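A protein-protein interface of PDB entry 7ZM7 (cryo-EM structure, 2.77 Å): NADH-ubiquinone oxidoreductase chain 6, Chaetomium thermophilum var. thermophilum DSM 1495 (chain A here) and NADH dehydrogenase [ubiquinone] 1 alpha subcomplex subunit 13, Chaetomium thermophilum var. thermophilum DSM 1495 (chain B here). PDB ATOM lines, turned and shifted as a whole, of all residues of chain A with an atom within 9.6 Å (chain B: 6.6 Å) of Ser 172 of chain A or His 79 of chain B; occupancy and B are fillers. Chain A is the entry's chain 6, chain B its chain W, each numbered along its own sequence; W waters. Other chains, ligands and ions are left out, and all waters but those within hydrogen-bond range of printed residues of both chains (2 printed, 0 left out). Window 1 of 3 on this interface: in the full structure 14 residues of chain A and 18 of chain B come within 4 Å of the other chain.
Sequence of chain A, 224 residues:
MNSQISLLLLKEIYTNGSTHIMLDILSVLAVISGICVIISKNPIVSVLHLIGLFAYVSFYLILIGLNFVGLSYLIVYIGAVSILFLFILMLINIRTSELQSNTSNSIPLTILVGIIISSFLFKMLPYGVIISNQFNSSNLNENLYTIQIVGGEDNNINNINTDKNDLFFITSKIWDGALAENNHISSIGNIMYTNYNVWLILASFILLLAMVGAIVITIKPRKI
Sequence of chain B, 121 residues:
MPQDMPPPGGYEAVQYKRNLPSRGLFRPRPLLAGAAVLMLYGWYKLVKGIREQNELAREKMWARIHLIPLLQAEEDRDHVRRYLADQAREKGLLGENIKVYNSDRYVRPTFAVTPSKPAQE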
ATOM      1  N   PHE A 169      -4.342  -8.451   4.381  1.00  0.00           N
ATOM      2  CA  PHE A 169      -4.658  -7.170   3.700  1.00  0.00           C
ATOM      3  C   PHE A 169      -4.666  -6.082   4.772  1.00  0.00           C
ATOM      4  O   PHE A 169      -5.101  -6.356   5.893  1.00  0.00           O
ATOM      5  CB  PHE A 169      -6.043  -7.239   3.057  1.00  0.00           C
ATOM      6  CG  PHE A 169      -6.104  -7.995   1.758  1.00  0.00           C
ATOM      7  CD1 PHE A 169      -5.701  -7.399   0.575  1.00  0.00           C
ATOM      8  CD2 PHE A 169      -6.576  -9.295   1.717  1.00  0.00           C
ATOM      9  CE1 PHE A 169      -5.765  -8.089  -0.624  1.00  0.00           C
ATOM     10  CE2 PHE A 169      -6.637  -9.985   0.518  1.00  0.00           C
ATOM     11  CZ  PHE A 169      -6.234  -9.379  -0.648  1.00  0.00           C
ATOM     12  N   ILE A 170      -4.184  -4.890   4.438  1.00  0.00           N
ATOM     13  CA  ILE A 170      -4.096  -3.789   5.439  1.00  0.00           C
ATOM     14  C   ILE A 170      -4.922  -2.603   4.945  1.00  0.00           C
ATOM     15  O   ILE A 170      -4.937  -2.373   3.727  1.00  0.00           O
ATOM     16  CB  ILE A 170      -2.625  -3.415   5.740  1.00  0.00           C
ATOM     17  CG1 ILE A 170      -2.498  -2.429   6.904  1.00  0.00           C
ATOM     18  CG2 ILE A 170      -1.895  -2.925   4.499  1.00  0.00           C
ATOM     19  CD1 ILE A 170      -2.177  -3.076   8.221  1.00  0.00           C
ATOM     20  N   THR A 171      -5.614  -1.912   5.852  1.00  0.00           N
ATOM     21  CA  THR A 171      -6.362  -0.689   5.466  1.00  0.00           C
ATOM     22  C   THR A 171      -6.094   0.450   6.453  1.00  0.00           C
ATOM     23  O   THR A 171      -5.824   0.153   7.622  1.00  0.00           O
ATOM     24  CB  THR A 171      -7.864  -0.944   5.297  1.00  0.00           C
ATOM     25  OG1 THR A 171      -8.327  -1.774   6.362  1.00  0.00           O
ATOM     26  CG2 THR A 171      -8.208  -1.549   3.955  1.00  0.00           C
ATOM     27  N   SER A 172      -6.180   1.697   5.988  1.00  0.00           N
ATOM     28  CA  SER A 172      -5.961   2.897   6.837  1.00  0.00           C
ATOM     29  C   SER A 172      -6.989   3.955   6.435  1.00  0.00           C
ATOM     30  O   SER A 172      -7.613   3.780   5.375  1.00  0.00           O
ATOM     31  CB  SER A 172      -4.564   3.410   6.685  1.00  0.00           C
ATOM     32  OG  SER A 172      -4.399   4.651   7.348  1.00  0.00           O
ATOM     33  N   LYS A 173      -7.168   5.000   7.246  1.00  0.00           N
ATOM     34  CA  LYS A 173      -8.207   6.030   6.980  1.00  0.00           C
ATOM     35  C   LYS A 173      -7.718   7.114   6.015  1.00  0.00           C
ATOM     36  O   LYS A 173      -6.498   7.227   5.833  1.00  0.00           O
ATOM     37  CB  LYS A 173      -8.660   6.639   8.311  1.00  0.00           C
ATOM     38  CG  LYS A 173      -7.563   7.220   9.187  1.00  0.00           C
ATOM     39  CD  LYS A 173      -8.060   7.734  10.517  1.00  0.00           C
ATOM     40  CE  LYS A 173      -8.647   6.653  11.399  1.00  0.00           C
ATOM     41  NZ  LYS A 173      -9.046   7.187  12.722  1.00  0.00           N
ATOM     42  N   ILE A 174      -8.643   7.860   5.403  1.00  0.00           N
ATOM     43  CA  ILE A 174      -8.311   9.008   4.503  1.00  0.00           C
ATOM     44  C   ILE A 174      -9.300  10.109   4.887  1.00  0.00           C
ATOM     45  O   ILE A 174     -10.363   9.769   5.411  1.00  0.00           O
ATOM     46  CB  ILE A 174      -8.453   8.613   3.018  1.00  0.00           C
ATOM     47  CG1 ILE A 174      -7.752   9.588   2.072  1.00  0.00           C
ATOM     48  CG2 ILE A 174      -9.910   8.408   2.632  1.00  0.00           C
ATOM     49  CD1 ILE A 174      -8.056   9.328   0.619  1.00  0.00           C
ATOM     50  N   TRP A 175      -8.948  11.376   4.692  1.00  0.00           N
ATOM     51  CA  TRP A 175      -9.840  12.467   5.149  1.00  0.00           C
ATOM     52  C   TRP A 175     -10.365  13.276   3.967  1.00  0.00           C
ATOM     53  O   TRP A 175     -11.565  13.564   3.938  1.00  0.00           O
ATOM     54  CB  TRP A 175      -9.113  13.322   6.183  1.00  0.00           C
ATOM     55  CG  TRP A 175      -8.811  12.572   7.442  1.00  0.00           C
ATOM     56  CD1 TRP A 175      -7.622  12.009   7.803  1.00  0.00           C
ATOM     57  CD2 TRP A 175      -9.732  12.271   8.505  1.00  0.00           C
ATOM     58  NE1 TRP A 175      -7.733  11.400   9.022  1.00  0.00           N
ATOM     59  CE2 TRP A 175      -9.016  11.542   9.476  1.00  0.00           C
ATOM     60  CE3 TRP A 175     -11.083  12.552   8.731  1.00  0.00           C
ATOM     61  CZ2 TRP A 175      -9.608  11.095  10.655  1.00  0.00           C
ATOM     62  CZ3 TRP A 175     -11.666  12.113   9.897  1.00  0.00           C
ATOM     63  CH2 TRP A 175     -10.936  11.398  10.844  1.00  0.00           C
ATOM     64  N   ASP A 176      -9.501  13.598   3.014  1.00  0.00           N
ATOM     65  CA  ASP A 176      -9.915  14.341   1.794  1.00  0.00           C
ATOM     66  C   ASP A 176     -10.923  13.509   0.995  1.00  0.00           C
ATOM     67  O   ASP A 176     -11.852  14.113   0.431  1.00  0.00           O
ATOM     68  CB  ASP A 176      -8.713  14.855   0.992  1.00  0.00           C
ATOM     69  CG  ASP A 176      -7.548  13.891   0.848  1.00  0.00           C
ATOM     70  OD1 ASP A 176      -7.762  12.676   1.000  1.00  0.00           O
ATOM     71  OD2 ASP A 176      -6.432  14.370   0.572  1.00  0.00           O
ATOM     72  N   ALA A 178     -12.973  11.271   2.278  1.00  0.00           N
ATOM     73  CA  ALA A 178     -14.114  10.895   3.145  1.00  0.00           C
ATOM     74  C   ALA A 178     -14.992  12.108   3.458  1.00  0.00           C
ATOM     75  O   ALA A 178     -15.773  12.011   4.395  1.00  0.00           O
ATOM     76  CB  ALA A 178     -13.599  10.268   4.415  1.00  0.00           C
ATOM     77  N   GLN B  72      -5.447  15.263   7.465  1.00  0.00           N
ATOM     78  CA  GLN B  72      -4.652  14.632   6.392  1.00  0.00           C
ATOM     79  C   GLN B  72      -3.167  14.725   6.720  1.00  0.00           C
ATOM     80  O   GLN B  72      -2.455  13.761   6.457  1.00  0.00           O
ATOM     81  CB  GLN B  72      -5.015  15.292   5.064  1.00  0.00           C
ATOM     82  CG  GLN B  72      -4.448  14.581   3.847  1.00  0.00           C
ATOM     83  CD  GLN B  72      -4.986  13.179   3.718  1.00  0.00           C
ATOM     84  OE1 GLN B  72      -6.153  12.906   3.988  1.00  0.00           O
ATOM     85  NE2 GLN B  72      -4.129  12.271   3.286  1.00  0.00           N
ATOM     86  N   GLU B  74      -1.672  14.783   9.608  1.00  0.00           N
ATOM     87  CA  GLU B  74      -1.327  13.779  10.632  1.00  0.00           C
ATOM     88  C   GLU B  74      -1.208  12.404   9.976  1.00  0.00           C
ATOM     89  O   GLU B  74      -0.256  11.689  10.307  1.00  0.00           O
ATOM     90  CB  GLU B  74      -2.416  13.806  11.692  1.00  0.00           C
ATOM     91  CG  GLU B  74      -2.064  12.995  12.917  1.00  0.00           C
ATOM     92  CD  GLU B  74      -3.256  12.366  13.608  1.00  0.00           C
ATOM     93  OE1 GLU B  74      -4.342  12.977  13.593  1.00  0.00           O
ATOM     94  OE2 GLU B  74      -3.093  11.261  14.140  1.00  0.00           O
ATOM     95  N   GLU B  75      -2.133  12.059   9.090  1.00  0.00           N
ATOM     96  CA  GLU B  75      -2.127  10.760   8.391  1.00  0.00           C
ATOM     97  C   GLU B  75      -0.897  10.653   7.498  1.00  0.00           C
ATOM     98  O   GLU B  75      -0.299   9.577   7.467  1.00  0.00           O
ATOM     99  CB  GLU B  75      -3.376  10.699   7.537  1.00  0.00           C
ATOM    100  CG  GLU B  75      -3.753   9.309   7.080  1.00  0.00           C
ATOM    101  CD  GLU B  75      -4.439   8.478   8.146  1.00  0.00           C
ATOM    102  OE1 GLU B  75      -4.989   9.077   9.092  1.00  0.00           O
ATOM    103  OE2 GLU B  75      -4.406   7.241   8.032  1.00  0.00           O
ATOM    104  N   ASP B  76      -0.533  11.740   6.826  1.00  0.00           N
ATOM    105  CA  ASP B  76       0.615  11.756   5.893  1.00  0.00           C
ATOM    106  C   ASP B  76       1.925  11.506   6.643  1.00  0.00           C
ATOM    107  O   ASP B  76       2.762  10.769   6.118  1.00  0.00           O
ATOM    108  CB  ASP B  76       0.586  13.037   5.063  1.00  0.00           C
ATOM    109  CG  ASP B  76      -0.504  13.016   4.011  1.00  0.00           C
ATOM    110  OD1 ASP B  76      -1.272  12.042   3.997  1.00  0.00           O
ATOM    111  OD2 ASP B  76      -0.567  13.964   3.207  1.00  0.00           O
ATOM    112  N   ARG B  77       2.088  12.101   7.828  1.00  0.00           N
ATOM    113  CA  ARG B  77       3.302  11.860   8.656  1.00  0.00           C
ATOM    114  C   ARG B  77       3.345  10.380   9.046  1.00  0.00           C
ATOM    115  O   ARG B  77       4.435   9.802   9.022  1.00  0.00           O
ATOM    116  CB  ARG B  77       3.361  12.823   9.845  1.00  0.00           C
ATOM    117  CG  ARG B  77       3.775  14.238   9.472  1.00  0.00           C
ATOM    118  CD  ARG B  77       3.827  15.147  10.681  1.00  0.00           C
ATOM    119  NE  ARG B  77       3.081  16.371  10.441  1.00  0.00           N
ATOM    120  CZ  ARG B  77       1.857  16.601  10.893  1.00  0.00           C
ATOM    121  NH1 ARG B  77       1.245  15.694  11.633  1.00  0.00           N
ATOM    122  NH2 ARG B  77       1.254  17.742  10.618  1.00  0.00           N
ATOM    123  N   ASP B  78       2.192   9.801   9.383  1.00  0.00           N
ATOM    124  CA  ASP B  78       2.084   8.367   9.759  1.00  0.00           C
ATOM    125  C   ASP B  78       2.363   7.471   8.543  1.00  0.00           C
ATOM    126  O   ASP B  78       2.956   6.417   8.735  1.00  0.00           O
ATOM    127  CB  ASP B  78       0.737   8.125  10.434  1.00  0.00           C
ATOM    128  CG  ASP B  78       0.652   6.835  11.225  1.00  0.00           C
ATOM    129  OD1 ASP B  78       1.192   6.809  12.346  1.00  0.00           O
ATOM    130  OD2 ASP B  78       0.032   5.879  10.724  1.00  0.00           O
ATOM    131  N   HIS B  79       1.904   7.857   7.353  1.00  0.00           N
ATOM    132  CA  HIS B  79       2.179   7.117   6.095  1.00  0.00           C
ATOM    133  C   HIS B  79       3.665   7.181   5.750  1.00  0.00           C
ATOM    134  O   HIS B  79       4.166   6.242   5.136  1.00  0.00           O
ATOM    135  CB  HIS B  79       1.262   7.577   4.955  1.00  0.00           C
ATOM    136  CG  HIS B  79      -0.088   6.950   5.013  1.00  0.00           C
ATOM    137  ND1 HIS B  79      -0.381   5.782   4.346  1.00  0.00           N
ATOM    138  CD2 HIS B  79      -1.206   7.299   5.674  1.00  0.00           C
ATOM    139  CE1 HIS B  79      -1.629   5.451   4.579  1.00  0.00           C
ATOM    140  NE2 HIS B  79      -2.155   6.361   5.395  1.00  0.00           N
ATOM    141  N   VAL B  80       4.328   8.265   6.123  1.00  0.00           N
ATOM    142  CA  VAL B  80       5.781   8.400   5.850  1.00  0.00           C
ATOM    143  C   VAL B  80       6.468   7.544   6.906  1.00  0.00           C
ATOM    144  O   VAL B  80       7.345   6.772   6.524  1.00  0.00           O
ATOM    145  CB  VAL B  80       6.225   9.876   5.918  1.00  0.00           C
ATOM    146  CG1 VAL B  80       7.730  10.044   6.026  1.00  0.00           C
ATOM    147  CG2 VAL B  80       5.664  10.699   4.773  1.00  0.00           C
ATOM    148  N   ARG B  81       6.030   7.629   8.161  1.00  0.00           N
ATOM    149  CA  ARG B  81       6.677   6.886   9.233  1.00  0.00           C
ATOM    150  C   ARG B  81       6.668   5.384   8.969  1.00  0.00           C
ATOM    151  O   ARG B  81       7.702   4.719   9.066  1.00  0.00           O
ATOM    152  CB  ARG B  81       5.984   7.203  10.553  1.00  0.00           C
ATOM    153  CG  ARG B  81       6.656   6.661  11.771  1.00  0.00           C
ATOM    154  CD  ARG B  81       5.902   7.034  13.023  1.00  0.00           C
ATOM    155  NE  ARG B  81       4.547   6.517  13.011  1.00  0.00           N
ATOM    156  CZ  ARG B  81       4.222   5.279  13.343  1.00  0.00           C
ATOM    157  NH1 ARG B  81       2.961   4.888  13.305  1.00  0.00           N
ATOM    158  NH2 ARG B  81       5.163   4.444  13.732  1.00  0.00           N
ATOM    159  N   ARG B  82       5.509   4.828   8.631  1.00  0.00           N
ATOM    160  CA  ARG B  82       5.423   3.387   8.458  1.00  0.00           C
ATOM    161  C   ARG B  82       6.053   2.935   7.157  1.00  0.00           C
ATOM    162  O   ARG B  82       6.505   1.793   7.063  1.00  0.00           O
ATOM    163  CB  ARG B  82       3.972   2.933   8.537  1.00  0.00           C
ATOM    164  CG  ARG B  82       3.317   3.274   9.846  1.00  0.00           C
ATOM    165  CD  ARG B  82       1.969   2.655   9.967  1.00  0.00           C
ATOM    166  NE  ARG B  82       2.021   1.205   9.958  1.00  0.00           N
ATOM    167  CZ  ARG B  82       1.307   0.449  10.769  1.00  0.00           C
ATOM    168  NH1 ARG B  82       1.400  -0.860  10.714  1.00  0.00           N
ATOM    169  NH2 ARG B  82       0.500   1.016  11.639  1.00  0.00           N
ATOM    170  N   TYR B  83       6.184   3.827   6.179  1.00  0.00           N
ATOM    171  CA  TYR B  83       6.820   3.438   4.902  1.00  0.00           C
ATOM    172  C   TYR B  83       8.330   3.424   5.070  1.00  0.00           C
ATOM    173  O   TYR B  83       8.966   2.487   4.590  1.00  0.00           O
ATOM    174  CB  TYR B  83       6.410   4.366   3.763  1.00  0.00           C
ATOM    175  CG  TYR B  83       7.194   4.163   2.492  1.00  0.00           C
ATOM    176  CD1 TYR B  83       6.800   3.222   1.558  1.00  0.00           C
ATOM    177  CD2 TYR B  83       8.341   4.892   2.231  1.00  0.00           C
ATOM    178  CE1 TYR B  83       7.523   3.013   0.398  1.00  0.00           C
ATOM    179  CE2 TYR B  83       9.077   4.695   1.078  1.00  0.00           C
ATOM    180  CZ  TYR B  83       8.665   3.753   0.157  1.00  0.00           C
ATOM    181  OH  TYR B  83       9.381   3.557  -0.988  1.00  0.00           O
ATOM    182  N   LEU B  84       8.870   4.392   5.798  1.00  0.00           N
ATOM    183  CA  LEU B  84      10.324   4.483   6.031  1.00  0.00           C
ATOM    184  C   LEU B  84      10.737   3.344   6.957  1.00  0.00           C
ATOM    185  O   LEU B  84      11.822   2.779   6.753  1.00  0.00           O
ATOM    186  CB  LEU B  84      10.613   5.877   6.586  1.00  0.00           C
ATOM    187  CG  LEU B  84      10.537   7.004   5.560  1.00  0.00           C
ATOM    188  CD1 LEU B  84      10.980   8.320   6.168  1.00  0.00           C
ATOM    189  CD2 LEU B  84      11.376   6.678   4.337  1.00  0.00           C
ATOM    190  N   TYR B 106       4.100   7.094  -4.288  1.00  0.00           N
ATOM    191  CA  TYR B 106       3.859   6.321  -3.057  1.00  0.00           C
ATOM    192  C   TYR B 106       2.517   5.635  -3.260  1.00  0.00           C
ATOM    193  O   TYR B 106       1.517   6.308  -3.507  1.00  0.00           O
ATOM    194  CB  TYR B 106       3.825   7.223  -1.820  1.00  0.00           C
ATOM    195  CG  TYR B 106       3.187   6.558  -0.631  1.00  0.00           C
ATOM    196  CD1 TYR B 106       3.777   5.454  -0.040  1.00  0.00           C
ATOM    197  CD2 TYR B 106       1.976   7.002  -0.132  1.00  0.00           C
ATOM    198  CE1 TYR B 106       3.183   4.812   1.030  1.00  0.00           C
ATOM    199  CE2 TYR B 106       1.370   6.373   0.937  1.00  0.00           C
ATOM    200  CZ  TYR B 106       1.980   5.279   1.519  1.00  0.00           C
ATOM    201  OH  TYR B 106       1.382   4.654   2.569  1.00  0.00           O
ATOM    202  N   ARG B 108      -0.373   3.379  -1.434  1.00  0.00           N
ATOM    203  CA  ARG B 108      -0.717   3.026  -0.034  1.00  0.00           C
ATOM    204  C   ARG B 108      -0.636   1.498   0.086  1.00  0.00           C
ATOM    205  O   ARG B 108      -1.322   0.849  -0.712  1.00  0.00           O
ATOM    206  CB  ARG B 108      -2.015   3.711   0.410  1.00  0.00           C
ATOM    207  CG  ARG B 108      -1.979   5.227   0.343  1.00  0.00           C
ATOM    208  CD  ARG B 108      -3.377   5.811   0.356  1.00  0.00           C
ATOM    209  NE  ARG B 108      -4.103   5.530   1.582  1.00  0.00           N
ATOM    210  CZ  ARG B 108      -4.169   6.348   2.623  1.00  0.00           C
ATOM    211  NH1 ARG B 108      -4.862   5.999   3.695  1.00  0.00           N
ATOM    212  NH2 ARG B 108      -3.532   7.505   2.595  1.00  0.00           N
ATOM    213  N   PRO B 109       0.130   0.879   1.025  1.00  0.00           N
ATOM    214  CA  PRO B 109       0.275  -0.590   1.041  1.00  0.00           C
ATOM    215  C   PRO B 109      -1.011  -1.431   1.046  1.00  0.00           C
ATOM    216  O   PRO B 109      -1.932  -1.027   1.669  1.00  0.00           O
ATOM    217  CB  PRO B 109       1.112  -0.793   2.301  1.00  0.00           C
ATOM    218  CG  PRO B 109       0.901   0.432   3.137  1.00  0.00           C
ATOM    219  CD  PRO B 109       0.822   1.542   2.123  1.00  0.00           C
HETATM  220  O   HOH W   1      -5.476   4.902  10.190  1.00  0.00           O
HETATM  221  O   HOH W   2      -4.045  11.950   0.242  1.00  0.00           O
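His 79 of chain B touches one residue of chain A. No residue of chain A comes within 4 Å of Asp 78 of chain B. Of the printed residues of chain A, Gln 72 of chain B touches Trp 175 and Asp 176. Of the printed residues of chain B, Asp 176 of chain A touches Gln 72. Asp 76 of chain B touches none of the printed residues of chain A. The nearest residue of chain B that does not touch Ser 172 of chain A is Asp 78 of chain B (5.7 Å).
NE2 of Gln 72 of chain B lies within hydrogen-bond range of OD1 of Asp 76 of chain B, at 3.0 Å. OH of Tyr 106 of chain B sits at hydrogen-bond distance from ND1 of His 79 of chain B. NE2 of His 79 of chain B sits at hydrogen-bond distance from NH1 of Arg 108 of chain B, at 3.2 Å.
OE1 of Gln 72 of chain B is in hydrogen-bond range of N of Trp 175 of chain A, at 3.3 Å. The side-chain amide oxygen (OE1) of Gln 72 of chain B sits close to the side-chain carboxylate (OD1) of Asp 176 of chain A (3.4 Å). The side-chain hydroxyl of Ser 172 of chain A is in hydrogen-bond range of the side-chain carboxylate of Glu 75 of chain B. A ring nitrogen (NE2) of His 79 of chain B lies within hydrogen-bond range of the side-chain hydroxyl (OG) of Ser 172 of chain A. The backbone carbonyl oxygen of Lys 173 of chain A sits at hydrogen-bond distance from the guanidinium group of Arg 108 of chain B, 3.0 Å away. O of Lys 173 of chain A sits close to OE2 of Glu 75 of chain B.
Water W1 lies within hydrogen-bond range of OG of Ser 172 of chain A (3.0 Å), OE2 of Glu 75 of chain B (3.4 Å) and N of Lys 173 of chain A (3.4 Å). Water W2 bridges NE2 of Gln 72 of chain B (3.1 Å) and OD2 of Asp 176 of chain A (3.4 Å).
Hydrophobic or aromatic side chains of chain A within 4 Å of the printed part of chain B: Ile 170 and Trp 175. Among the printed residues, 9 pairs touch across the chains.
Among the printed residues, merely in contact across the chains: Ile 170 of chain A with Pro 109 of chain B, Trp 175 of chain A with Glu 75 of chain B and Ser 172 of chain A with Arg 108 of chain B.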
